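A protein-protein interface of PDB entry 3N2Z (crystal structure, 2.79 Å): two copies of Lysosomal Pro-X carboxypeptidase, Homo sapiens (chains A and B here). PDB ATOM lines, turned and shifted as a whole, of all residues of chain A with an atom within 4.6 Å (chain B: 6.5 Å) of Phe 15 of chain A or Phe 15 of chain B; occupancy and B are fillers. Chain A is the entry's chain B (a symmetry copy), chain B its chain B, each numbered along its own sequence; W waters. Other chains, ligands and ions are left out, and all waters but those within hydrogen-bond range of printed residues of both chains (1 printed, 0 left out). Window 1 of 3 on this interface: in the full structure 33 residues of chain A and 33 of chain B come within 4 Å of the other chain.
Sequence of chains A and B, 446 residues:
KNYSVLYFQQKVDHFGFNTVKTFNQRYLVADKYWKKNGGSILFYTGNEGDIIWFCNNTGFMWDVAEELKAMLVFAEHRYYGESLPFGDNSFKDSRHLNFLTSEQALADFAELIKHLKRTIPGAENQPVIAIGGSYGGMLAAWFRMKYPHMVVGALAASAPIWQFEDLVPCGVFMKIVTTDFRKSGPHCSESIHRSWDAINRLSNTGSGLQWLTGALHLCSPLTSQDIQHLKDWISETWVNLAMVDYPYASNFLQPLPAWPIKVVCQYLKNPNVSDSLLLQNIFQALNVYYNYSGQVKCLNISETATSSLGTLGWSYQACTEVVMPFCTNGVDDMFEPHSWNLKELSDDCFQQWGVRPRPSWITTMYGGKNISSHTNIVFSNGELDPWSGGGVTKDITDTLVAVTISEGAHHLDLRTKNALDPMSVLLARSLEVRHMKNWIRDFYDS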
ATOM      1  N   ASP A  13       6.256  -3.044 -19.722  1.00  0.00           N
ATOM      2  CA  ASP A  13       6.979  -1.775 -19.694  1.00  0.00           C
ATOM      3  C   ASP A  13       8.096  -1.706 -20.748  1.00  0.00           C
ATOM      4  O   ASP A  13       9.054  -2.481 -20.683  1.00  0.00           O
ATOM      5  CB  ASP A  13       7.522  -1.511 -18.282  1.00  0.00           C
ATOM      6  CG  ASP A  13       8.034  -0.120 -18.042  1.00  0.00           C
ATOM      7  OD1 ASP A  13       8.008   0.697 -18.989  1.00  0.00           O
ATOM      8  OD2 ASP A  13       8.452   0.165 -16.909  1.00  0.00           O
ATOM      9  N   HIS A  14       7.981  -0.768 -21.712  1.00  0.00           N
ATOM     10  CA  HIS A  14       9.004  -0.598 -22.751  1.00  0.00           C
ATOM     11  C   HIS A  14      10.022   0.460 -22.305  1.00  0.00           C
ATOM     12  O   HIS A  14      11.169   0.492 -22.790  1.00  0.00           O
ATOM     13  CB  HIS A  14       8.367  -0.180 -24.073  1.00  0.00           C
ATOM     14  CG  HIS A  14       7.404  -1.170 -24.636  1.00  0.00           C
ATOM     15  ND1 HIS A  14       7.839  -2.265 -25.353  1.00  0.00           N
ATOM     16  CD2 HIS A  14       6.051  -1.162 -24.627  1.00  0.00           C
ATOM     17  CE1 HIS A  14       6.739  -2.906 -25.730  1.00  0.00           C
ATOM     18  NE2 HIS A  14       5.641  -2.272 -25.322  1.00  0.00           N
ATOM     19  N   PHE A  15       9.603   1.298 -21.347  1.00  0.00           N
ATOM     20  CA  PHE A  15      10.412   2.390 -20.829  1.00  0.00           C
ATOM     21  C   PHE A  15      11.196   2.136 -19.540  1.00  0.00           C
ATOM     22  O   PHE A  15      11.843   3.050 -19.011  1.00  0.00           O
ATOM     23  CB  PHE A  15       9.630   3.723 -20.878  1.00  0.00           C
ATOM     24  CG  PHE A  15       8.997   3.933 -22.248  1.00  0.00           C
ATOM     25  CD1 PHE A  15       9.738   4.456 -23.303  1.00  0.00           C
ATOM     26  CD2 PHE A  15       7.677   3.547 -22.494  1.00  0.00           C
ATOM     27  CE1 PHE A  15       9.176   4.593 -24.575  1.00  0.00           C
ATOM     28  CE2 PHE A  15       7.117   3.677 -23.769  1.00  0.00           C
ATOM     29  CZ  PHE A  15       7.872   4.199 -24.806  1.00  0.00           C
ATOM     30  N   GLY A  16      11.183   0.887 -19.074  1.00  0.00           N
ATOM     31  CA  GLY A  16      11.868   0.501 -17.849  1.00  0.00           C
ATOM     32  C   GLY A  16      12.292  -0.937 -17.815  1.00  0.00           C
ATOM     33  O   GLY A  16      11.652  -1.793 -18.427  1.00  0.00           O
ATOM     34  N   ASN A  98      -0.251   2.366 -14.423  1.00  0.00           N
ATOM     35  CA  ASN A  98       0.954   3.113 -14.753  1.00  0.00           C
ATOM     36  C   ASN A  98       1.317   2.977 -16.247  1.00  0.00           C
ATOM     37  O   ASN A  98       1.627   3.986 -16.881  1.00  0.00           O
ATOM     38  CB  ASN A  98       2.097   2.648 -13.847  1.00  0.00           C
ATOM     39  CG  ASN A  98       3.355   3.480 -13.916  1.00  0.00           C
ATOM     40  OD1 ASN A  98       3.373   4.693 -13.651  1.00  0.00           O
ATOM     41  ND2 ASN A  98       4.447   2.834 -14.259  1.00  0.00           N
ATOM     42  N   THR A 101      -0.270   4.536 -21.429  1.00  0.00           N
ATOM     43  CA  THR A 101       0.180   5.786 -22.046  1.00  0.00           C
ATOM     44  C   THR A 101       0.161   5.594 -23.562  1.00  0.00           C
ATOM     45  O   THR A 101       0.099   4.449 -24.053  1.00  0.00           O
ATOM     46  CB  THR A 101       1.591   6.221 -21.576  1.00  0.00           C
ATOM     47  OG1 THR A 101       2.615   5.351 -22.098  1.00  0.00           O
ATOM     48  CG2 THR A 101       1.700   6.435 -20.079  1.00  0.00           C
ATOM     49  N   GLU A 103       2.764   6.498 -25.500  1.00  0.00           N
ATOM     50  CA  GLU A 103       4.116   6.026 -25.817  1.00  0.00           C
ATOM     51  C   GLU A 103       4.181   4.512 -25.737  1.00  0.00           C
ATOM     52  O   GLU A 103       4.688   3.873 -26.670  1.00  0.00           O
ATOM     53  CB  GLU A 103       5.187   6.646 -24.911  1.00  0.00           C
ATOM     54  CG  GLU A 103       5.327   8.164 -24.993  1.00  0.00           C
ATOM     55  CD  GLU A 103       4.308   8.991 -24.229  1.00  0.00           C
ATOM     56  OE1 GLU A 103       3.336   8.404 -23.701  1.00  0.00           O
ATOM     57  OE2 GLU A 103       4.480  10.231 -24.163  1.00  0.00           O
ATOM     58  N   GLN A 104       3.620   3.922 -24.665  1.00  0.00           N
ATOM     59  CA  GLN A 104       3.595   2.461 -24.512  1.00  0.00           C
ATOM     60  C   GLN A 104       2.843   1.825 -25.670  1.00  0.00           C
ATOM     61  O   GLN A 104       3.349   0.870 -26.238  1.00  0.00           O
ATOM     62  CB  GLN A 104       3.015   2.019 -23.161  1.00  0.00           C
ATOM     63  CG  GLN A 104       3.778   2.502 -21.927  1.00  0.00           C
ATOM     64  CD  GLN A 104       4.929   1.633 -21.481  1.00  0.00           C
ATOM     65  OE1 GLN A 104       5.411   0.737 -22.193  1.00  0.00           O
ATOM     66  NE2 GLN A 104       5.400   1.905 -20.269  1.00  0.00           N
ATOM     67  N   ALA A 107       4.972   2.051 -28.818  1.00  0.00           N
ATOM     68  CA  ALA A 107       6.043   1.068 -28.671  1.00  0.00           C
ATOM     69  C   ALA A 107       5.483  -0.349 -28.956  1.00  0.00           C
ATOM     70  O   ALA A 107       6.178  -1.140 -29.600  1.00  0.00           O
ATOM     71  CB  ALA A 107       6.637   1.154 -27.283  1.00  0.00           C
ATOM     72  N   TRP A 361       2.409  18.000 -21.430  1.00  0.00           N
ATOM     73  CA  TRP A 361       3.125  16.827 -21.893  1.00  0.00           C
ATOM     74  C   TRP A 361       3.073  16.495 -23.385  1.00  0.00           C
ATOM     75  O   TRP A 361       4.125  16.489 -24.016  1.00  0.00           O
ATOM     76  CB  TRP A 361       2.892  15.610 -20.991  1.00  0.00           C
ATOM     77  CG  TRP A 361       3.675  14.399 -21.426  1.00  0.00           C
ATOM     78  CD1 TRP A 361       3.162  13.194 -21.814  1.00  0.00           C
ATOM     79  CD2 TRP A 361       5.103  14.282 -21.531  1.00  0.00           C
ATOM     80  NE1 TRP A 361       4.179  12.334 -22.153  1.00  0.00           N
ATOM     81  CE2 TRP A 361       5.384  12.968 -21.971  1.00  0.00           C
ATOM     82  CE3 TRP A 361       6.176  15.163 -21.308  1.00  0.00           C
ATOM     83  CZ2 TRP A 361       6.693  12.511 -22.183  1.00  0.00           C
ATOM     84  CZ3 TRP A 361       7.475  14.716 -21.537  1.00  0.00           C
ATOM     85  CH2 TRP A 361       7.721  13.400 -21.951  1.00  0.00           C
ATOM     86  N   VAL B  12      10.847  12.581 -12.035  1.00  0.00           N
ATOM     87  CA  VAL B  12      11.704  11.397 -12.059  1.00  0.00           C
ATOM     88  C   VAL B  12      11.252  10.512 -13.212  1.00  0.00           C
ATOM     89  O   VAL B  12      12.086  10.026 -13.969  1.00  0.00           O
ATOM     90  CB  VAL B  12      11.748  10.680 -10.673  1.00  0.00           C
ATOM     91  CG1 VAL B  12      12.215   9.236 -10.776  1.00  0.00           C
ATOM     92  CG2 VAL B  12      12.629  11.454  -9.701  1.00  0.00           C
ATOM     93  N   ASP B  13       9.933  10.361 -13.379  1.00  0.00           N
ATOM     94  CA  ASP B  13       9.360   9.542 -14.444  1.00  0.00           C
ATOM     95  C   ASP B  13       8.542  10.366 -15.450  1.00  0.00           C
ATOM     96  O   ASP B  13       7.521  10.952 -15.082  1.00  0.00           O
ATOM     97  CB  ASP B  13       8.525   8.403 -13.839  1.00  0.00           C
ATOM     98  CG  ASP B  13       8.118   7.326 -14.802  1.00  0.00           C
ATOM     99  OD1 ASP B  13       8.455   7.440 -16.002  1.00  0.00           O
ATOM    100  OD2 ASP B  13       7.472   6.361 -14.365  1.00  0.00           O
ATOM    101  N   HIS B  14       8.981  10.399 -16.726  1.00  0.00           N
ATOM    102  CA  HIS B  14       8.260  11.133 -17.774  1.00  0.00           C
ATOM    103  C   HIS B  14       7.280  10.190 -18.484  1.00  0.00           C
ATOM    104  O   HIS B  14       6.293  10.635 -19.100  1.00  0.00           O
ATOM    105  CB  HIS B  14       9.236  11.727 -18.785  1.00  0.00           C
ATOM    106  CG  HIS B  14      10.197  12.713 -18.213  1.00  0.00           C
ATOM    107  ND1 HIS B  14       9.835  14.028 -18.001  1.00  0.00           N
ATOM    108  CD2 HIS B  14      11.502  12.560 -17.889  1.00  0.00           C
ATOM    109  CE1 HIS B  14      10.921  14.625 -17.525  1.00  0.00           C
ATOM    110  NE2 HIS B  14      11.949  13.781 -17.449  1.00  0.00           N
ATOM    111  N   PHE B  15       7.542   8.882 -18.357  1.00  0.00           N
ATOM    112  CA  PHE B  15       6.751   7.842 -18.995  1.00  0.00           C
ATOM    113  C   PHE B  15       5.659   7.174 -18.158  1.00  0.00           C
ATOM    114  O   PHE B  15       5.003   6.233 -18.623  1.00  0.00           O
ATOM    115  CB  PHE B  15       7.656   6.877 -19.796  1.00  0.00           C
ATOM    116  CG  PHE B  15       8.618   7.650 -20.692  1.00  0.00           C
ATOM    117  CD1 PHE B  15       8.209   8.122 -21.935  1.00  0.00           C
ATOM    118  CD2 PHE B  15       9.910   7.955 -20.260  1.00  0.00           C
ATOM    119  CE1 PHE B  15       9.071   8.882 -22.731  1.00  0.00           C
ATOM    120  CE2 PHE B  15      10.770   8.721 -21.053  1.00  0.00           C
ATOM    121  CZ  PHE B  15      10.344   9.184 -22.287  1.00  0.00           C
ATOM    122  N   GLY B  16       5.430   7.699 -16.954  1.00  0.00           N
ATOM    123  CA  GLY B  16       4.436   7.158 -16.040  1.00  0.00           C
ATOM    124  C   GLY B  16       3.868   8.168 -15.088  1.00  0.00           C
ATOM    125  O   GLY B  16       4.544   9.131 -14.721  1.00  0.00           O
ATOM    126  N   PHE B  17       2.619   7.940 -14.677  1.00  0.00           N
ATOM    127  CA  PHE B  17       1.918   8.848 -13.774  1.00  0.00           C
ATOM    128  C   PHE B  17       1.898   8.462 -12.296  1.00  0.00           C
ATOM    129  O   PHE B  17       1.616   9.326 -11.461  1.00  0.00           O
ATOM    130  CB  PHE B  17       0.528   9.214 -14.340  1.00  0.00           C
ATOM    131  CG  PHE B  17       0.652  10.145 -15.523  1.00  0.00           C
ATOM    132  CD1 PHE B  17       0.622  11.522 -15.346  1.00  0.00           C
ATOM    133  CD2 PHE B  17       0.882   9.641 -16.805  1.00  0.00           C
ATOM    134  CE1 PHE B  17       0.763  12.382 -16.436  1.00  0.00           C
ATOM    135  CE2 PHE B  17       1.046  10.497 -17.890  1.00  0.00           C
ATOM    136  CZ  PHE B  17       0.978  11.864 -17.701  1.00  0.00           C
ATOM    137  N   ASN B  98      15.506   2.157 -12.231  1.00  0.00           N
ATOM    138  CA  ASN B  98      14.500   2.003 -13.271  1.00  0.00           C
ATOM    139  C   ASN B  98      14.493   3.206 -14.239  1.00  0.00           C
ATOM    140  O   ASN B  98      14.451   2.999 -15.452  1.00  0.00           O
ATOM    141  CB  ASN B  98      13.131   1.794 -12.620  1.00  0.00           C
ATOM    142  CG  ASN B  98      12.020   1.400 -13.562  1.00  0.00           C
ATOM    143  OD1 ASN B  98      12.065   0.376 -14.264  1.00  0.00           O
ATOM    144  ND2 ASN B  98      10.981   2.205 -13.585  1.00  0.00           N
ATOM    145  N   PHE B  99      14.616   4.436 -13.701  1.00  0.00           N
ATOM    146  CA  PHE B  99      14.581   5.702 -14.437  1.00  0.00           C
ATOM    147  C   PHE B  99      15.820   6.152 -15.221  1.00  0.00           C
ATOM    148  O   PHE B  99      15.831   7.260 -15.771  1.00  0.00           O
ATOM    149  CB  PHE B  99      13.975   6.808 -13.562  1.00  0.00           C
ATOM    150  CG  PHE B  99      12.788   6.252 -12.806  1.00  0.00           C
ATOM    151  CD1 PHE B  99      11.621   5.891 -13.477  1.00  0.00           C
ATOM    152  CD2 PHE B  99      12.873   5.993 -11.440  1.00  0.00           C
ATOM    153  CE1 PHE B  99      10.548   5.332 -12.787  1.00  0.00           C
ATOM    154  CE2 PHE B  99      11.790   5.447 -10.749  1.00  0.00           C
ATOM    155  CZ  PHE B  99      10.640   5.111 -11.429  1.00  0.00           C
ATOM    156  N   THR B 101      17.429   5.684 -18.368  1.00  0.00           N
ATOM    157  CA  THR B 101      17.273   5.312 -19.775  1.00  0.00           C
ATOM    158  C   THR B 101      17.634   6.530 -20.626  1.00  0.00           C
ATOM    159  O   THR B 101      17.693   7.664 -20.111  1.00  0.00           O
ATOM    160  CB  THR B 101      15.843   4.822 -20.118  1.00  0.00           C
ATOM    161  OG1 THR B 101      14.889   5.902 -20.082  1.00  0.00           O
ATOM    162  CG2 THR B 101      15.401   3.612 -19.318  1.00  0.00           C
ATOM    163  N   SER B 102      17.851   6.300 -21.936  1.00  0.00           N
ATOM    164  CA  SER B 102      18.157   7.387 -22.860  1.00  0.00           C
ATOM    165  C   SER B 102      16.888   8.216 -23.128  1.00  0.00           C
ATOM    166  O   SER B 102      17.000   9.445 -23.229  1.00  0.00           O
ATOM    167  CB  SER B 102      18.794   6.866 -24.138  1.00  0.00           C
ATOM    168  OG  SER B 102      18.023   5.823 -24.706  1.00  0.00           O
ATOM    169  N   GLU B 103      15.680   7.567 -23.166  1.00  0.00           N
ATOM    170  CA  GLU B 103      14.402   8.259 -23.359  1.00  0.00           C
ATOM    171  C   GLU B 103      14.162   9.252 -22.236  1.00  0.00           C
ATOM    172  O   GLU B 103      13.830  10.415 -22.510  1.00  0.00           O
ATOM    173  CB  GLU B 103      13.215   7.294 -23.468  1.00  0.00           C
ATOM    174  CG  GLU B 103      13.257   6.321 -24.643  1.00  0.00           C
ATOM    175  CD  GLU B 103      14.144   5.098 -24.492  1.00  0.00           C
ATOM    176  OE1 GLU B 103      14.894   5.023 -23.492  1.00  0.00           O
ATOM    177  OE2 GLU B 103      14.091   4.214 -25.380  1.00  0.00           O
ATOM    178  N   GLN B 104      14.386   8.831 -20.977  1.00  0.00           N
ATOM    179  CA  GLN B 104      14.222   9.727 -19.823  1.00  0.00           C
ATOM    180  C   GLN B 104      15.159  10.917 -19.944  1.00  0.00           C
ATOM    181  O   GLN B 104      14.707  12.035 -19.753  1.00  0.00           O
ATOM    182  CB  GLN B 104      14.412   9.002 -18.484  1.00  0.00           C
ATOM    183  CG  GLN B 104      13.429   7.863 -18.205  1.00  0.00           C
ATOM    184  CD  GLN B 104      12.121   8.262 -17.566  1.00  0.00           C
ATOM    185  OE1 GLN B 104      11.734   9.440 -17.504  1.00  0.00           O
ATOM    186  NE2 GLN B 104      11.404   7.254 -17.080  1.00  0.00           N
ATOM    187  N   ALA B 105      16.430  10.694 -20.321  1.00  0.00           N
ATOM    188  CA  ALA B 105      17.426  11.768 -20.531  1.00  0.00           C
ATOM    189  C   ALA B 105      16.967  12.736 -21.645  1.00  0.00           C
ATOM    190  O   ALA B 105      16.989  13.954 -21.445  1.00  0.00           O
ATOM    191  CB  ALA B 105      18.785  11.174 -20.876  1.00  0.00           C
ATOM    192  N   ALA B 107      13.882  13.240 -22.677  1.00  0.00           N
ATOM    193  CA  ALA B 107      12.710  13.924 -22.133  1.00  0.00           C
ATOM    194  C   ALA B 107      13.173  15.046 -21.169  1.00  0.00           C
ATOM    195  O   ALA B 107      12.574  16.125 -21.189  1.00  0.00           O
ATOM    196  CB  ALA B 107      11.813  12.931 -21.428  1.00  0.00           C
ATOM    197  N   TYR B 147      12.848  14.757 -31.167  1.00  0.00           N
ATOM    198  CA  TYR B 147      12.331  16.074 -30.818  1.00  0.00           C
ATOM    199  C   TYR B 147      12.769  17.150 -31.858  1.00  0.00           C
ATOM    200  O   TYR B 147      13.471  18.108 -31.489  1.00  0.00           O
ATOM    201  CB  TYR B 147      12.715  16.438 -29.363  1.00  0.00           C
ATOM    202  CG  TYR B 147      12.239  15.449 -28.311  1.00  0.00           C
ATOM    203  CD1 TYR B 147      11.181  15.762 -27.458  1.00  0.00           C
ATOM    204  CD2 TYR B 147      12.884  14.226 -28.129  1.00  0.00           C
ATOM    205  CE1 TYR B 147      10.753  14.866 -26.475  1.00  0.00           C
ATOM    206  CE2 TYR B 147      12.445  13.311 -27.171  1.00  0.00           C
ATOM    207  CZ  TYR B 147      11.388  13.640 -26.335  1.00  0.00           C
ATOM    208  OH  TYR B 147      10.967  12.740 -25.375  1.00  0.00           O
ATOM    209  N   GLU B 321      19.812  -0.975 -22.285  1.00  0.00           N
ATOM    210  CA  GLU B 321      19.595  -0.455 -23.647  1.00  0.00           C
ATOM    211  C   GLU B 321      20.819  -0.510 -24.581  1.00  0.00           C
ATOM    212  O   GLU B 321      20.745  -1.074 -25.682  1.00  0.00           O
ATOM    213  CB  GLU B 321      19.127   1.007 -23.564  1.00  0.00           C
ATOM    214  CG  GLU B 321      17.735   1.201 -23.011  1.00  0.00           C
ATOM    215  CD  GLU B 321      17.130   2.571 -23.230  1.00  0.00           C
ATOM    216  OE1 GLU B 321      17.878   3.576 -23.219  1.00  0.00           O
ATOM    217  OE2 GLU B 321      15.893   2.632 -23.405  1.00  0.00           O
ATOM    218  N   ARG B 358      18.121  -5.814 -23.445  1.00  0.00           N
ATOM    219  CA  ARG B 358      17.159  -5.879 -24.543  1.00  0.00           C
ATOM    220  C   ARG B 358      18.020  -5.488 -25.768  1.00  0.00           C
ATOM    221  O   ARG B 358      18.183  -4.313 -26.082  1.00  0.00           O
ATOM    222  CB  ARG B 358      15.931  -4.997 -24.280  1.00  0.00           C
ATOM    223  CG  ARG B 358      14.888  -5.704 -23.401  1.00  0.00           C
ATOM    224  CD  ARG B 358      13.798  -4.761 -22.931  1.00  0.00           C
ATOM    225  NE  ARG B 358      13.297  -5.065 -21.587  1.00  0.00           N
ATOM    226  CZ  ARG B 358      12.441  -4.298 -20.910  1.00  0.00           C
ATOM    227  NH1 ARG B 358      11.993  -3.166 -21.437  1.00  0.00           N
ATOM    228  NH2 ARG B 358      12.028  -4.655 -19.702  1.00  0.00           N
ATOM    229  N   TRP B 361      16.242  -3.315 -28.666  1.00  0.00           N
ATOM    230  CA  TRP B 361      15.540  -2.101 -28.300  1.00  0.00           C
ATOM    231  C   TRP B 361      15.913  -0.807 -29.025  1.00  0.00           C
ATOM    232  O   TRP B 361      15.048  -0.241 -29.686  1.00  0.00           O
ATOM    233  CB  TRP B 361      15.422  -1.933 -26.781  1.00  0.00           C
ATOM    234  CG  TRP B 361      14.645  -0.705 -26.384  1.00  0.00           C
ATOM    235  CD1 TRP B 361      15.108   0.351 -25.651  1.00  0.00           C
ATOM    236  CD2 TRP B 361      13.279  -0.401 -26.712  1.00  0.00           C
ATOM    237  NE1 TRP B 361      14.118   1.292 -25.500  1.00  0.00           N
ATOM    238  CE2 TRP B 361      12.977   0.849 -26.124  1.00  0.00           C
ATOM    239  CE3 TRP B 361      12.281  -1.056 -27.455  1.00  0.00           C
ATOM    240  CZ2 TRP B 361      11.717   1.452 -26.249  1.00  0.00           C
ATOM    241  CZ3 TRP B 361      11.037  -0.449 -27.595  1.00  0.00           C
ATOM    242  CH2 TRP B 361      10.761   0.780 -26.981  1.00  0.00           C
ATOM    243  N   MET B 365      13.525   1.646 -31.240  1.00  0.00           N
ATOM    244  CA  MET B 365      13.243   3.011 -30.836  1.00  0.00           C
ATOM    245  C   MET B 365      13.795   4.056 -31.850  1.00  0.00           C
ATOM    246  O   MET B 365      13.019   4.779 -32.483  1.00  0.00           O
ATOM    247  CB  MET B 365      13.769   3.246 -29.405  1.00  0.00           C
ATOM    248  CG  MET B 365      13.529   4.650 -28.862  1.00  0.00           C
ATOM    249  SD  MET B 365      11.780   4.985 -28.566  1.00  0.00           S
ATOM    250  CE  MET B 365      11.888   6.611 -27.860  1.00  0.00           C
HETATM  251  O   HOH W   1      12.075  -1.824 -24.035  1.00  0.00           O
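The backbone carbonyl oxygen (O) of Asp 13 of chain A is in hydrogen-bond range of the guanidinium group (NH1) of Arg 358 of chain B, 3.1 Å away. The side-chain amide oxygen of Asn 98 of chain A lies within hydrogen-bond range of the backbone NH of Phe 17 of chain B, at 3.5 Å. The guanidinium group (NH2) of Arg 358 of chain B lies within hydrogen-bond range of the backbone carbonyl oxygen (O) of Gly 16 of chain A.
Of the printed residues of chain B, Asp 13 of chain A touches Arg 358. Of the printed residues of chain B, Thr 101 of chain A touches Phe 15. Printed residues of chain A within 4 Å of Phe 15 of chain B: Phe 15 (3.9 Å) and Thr 101 (3.6 Å). Of the printed residues of chain A, Trp 361 of chain B touches His 14 (3.6 Å). The nearest residue of chain B that does not touch Phe 15 of chain A is Glu 103 of chain B (4.2 Å).
His 14 of chain A touches Arg 358 of chain B (O to NH1, 3.99 Å). His 14 of chain A touches Trp 361 of chain B. Phe 15 of chain A touches Phe 15 of chain B. Thr 101 of chain B touches Phe 15 of chain A (CG2 to O, 3.6 Å). Asn 98 of chain B touches Gly 16 of chain A. OD1 of Asn 98 of chain A touches CA of Gly 16 of chain B, at 3.6 Å. O of Phe 15 of chain B touches CG2 of Thr 101 of chain A, at 3.6 Å. CZ2 of Trp 361 of chain A touches O of His 14 of chain B, 3.6 Å away.
Of the 10 printed residues of chain A, 7 touch a printed residue of chain B. Printed residues of chain A that touch a printed residue of chain B: Asp 13, His 14, Phe 15, Gly 16, Asn 98, Thr 101 and Trp 361. Hydrophobic or aromatic side chains of chain B within 4 Å of the printed part of chain A: His 14, Phe 15 and Trp 361. Among the printed residues, no Asp or Glu carboxylate lies within 4 Å of a Lys or Arg side-chain nitrogen of the other chain.
Water W1 bridges O of His 14 of chain A (2.8 Å) and NH1 of Arg 358 of chain B (2.9 Å).
His 14 of chain A touches Trp 361 of chain B, and with the chains exchanged Trp 361 of chain A touches His 14 of chain B. Phe 15 of chain A touches its own counterpart, Phe 15 of chain B. Phe 15 of chain A touches Thr 101 of chain B, and with the chains exchanged Thr 101 of chain A touches Phe 15 of chain B. Gly 16 of chain A touches Asn 98 of chain B, and with the chains exchanged Asn 98 of chain A touches Gly 16 of chain B. Of the 11 pairs that touch across the chains among the printed residues, 7 have their exchanged pair printed and touching as well.
The side-chain carboxylate (OE2) of Glu 103 of chain B is in hydrogen-bond range of the indole nitrogen (NE1) of Trp 361 of chain B, at 2.9 Å. NE1 of Trp 361 of chain B sits at hydrogen-bond distance from OE2 of Glu 321 of chain B (3.1 Å). OD1 of Asp 13 of chain B is in hydrogen-bond range of N of Phe 15 of chain B, at 2.9 Å. The side-chain carboxylate (OD1) of Asp 13 of chain A sits at hydrogen-bond distance from the backbone NH (N) of Phe 15 of chain A (2.9 Å). The side-chain carboxylate of Glu 103 of chain A sits at hydrogen-bond distance from the indole nitrogen of Trp 361 of chain A. The side-chain hydroxyl (OG1) of Thr 101 of chain B sits close to the backbone NH (N) of Gln 104 of chain B, at 3.1 Å.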
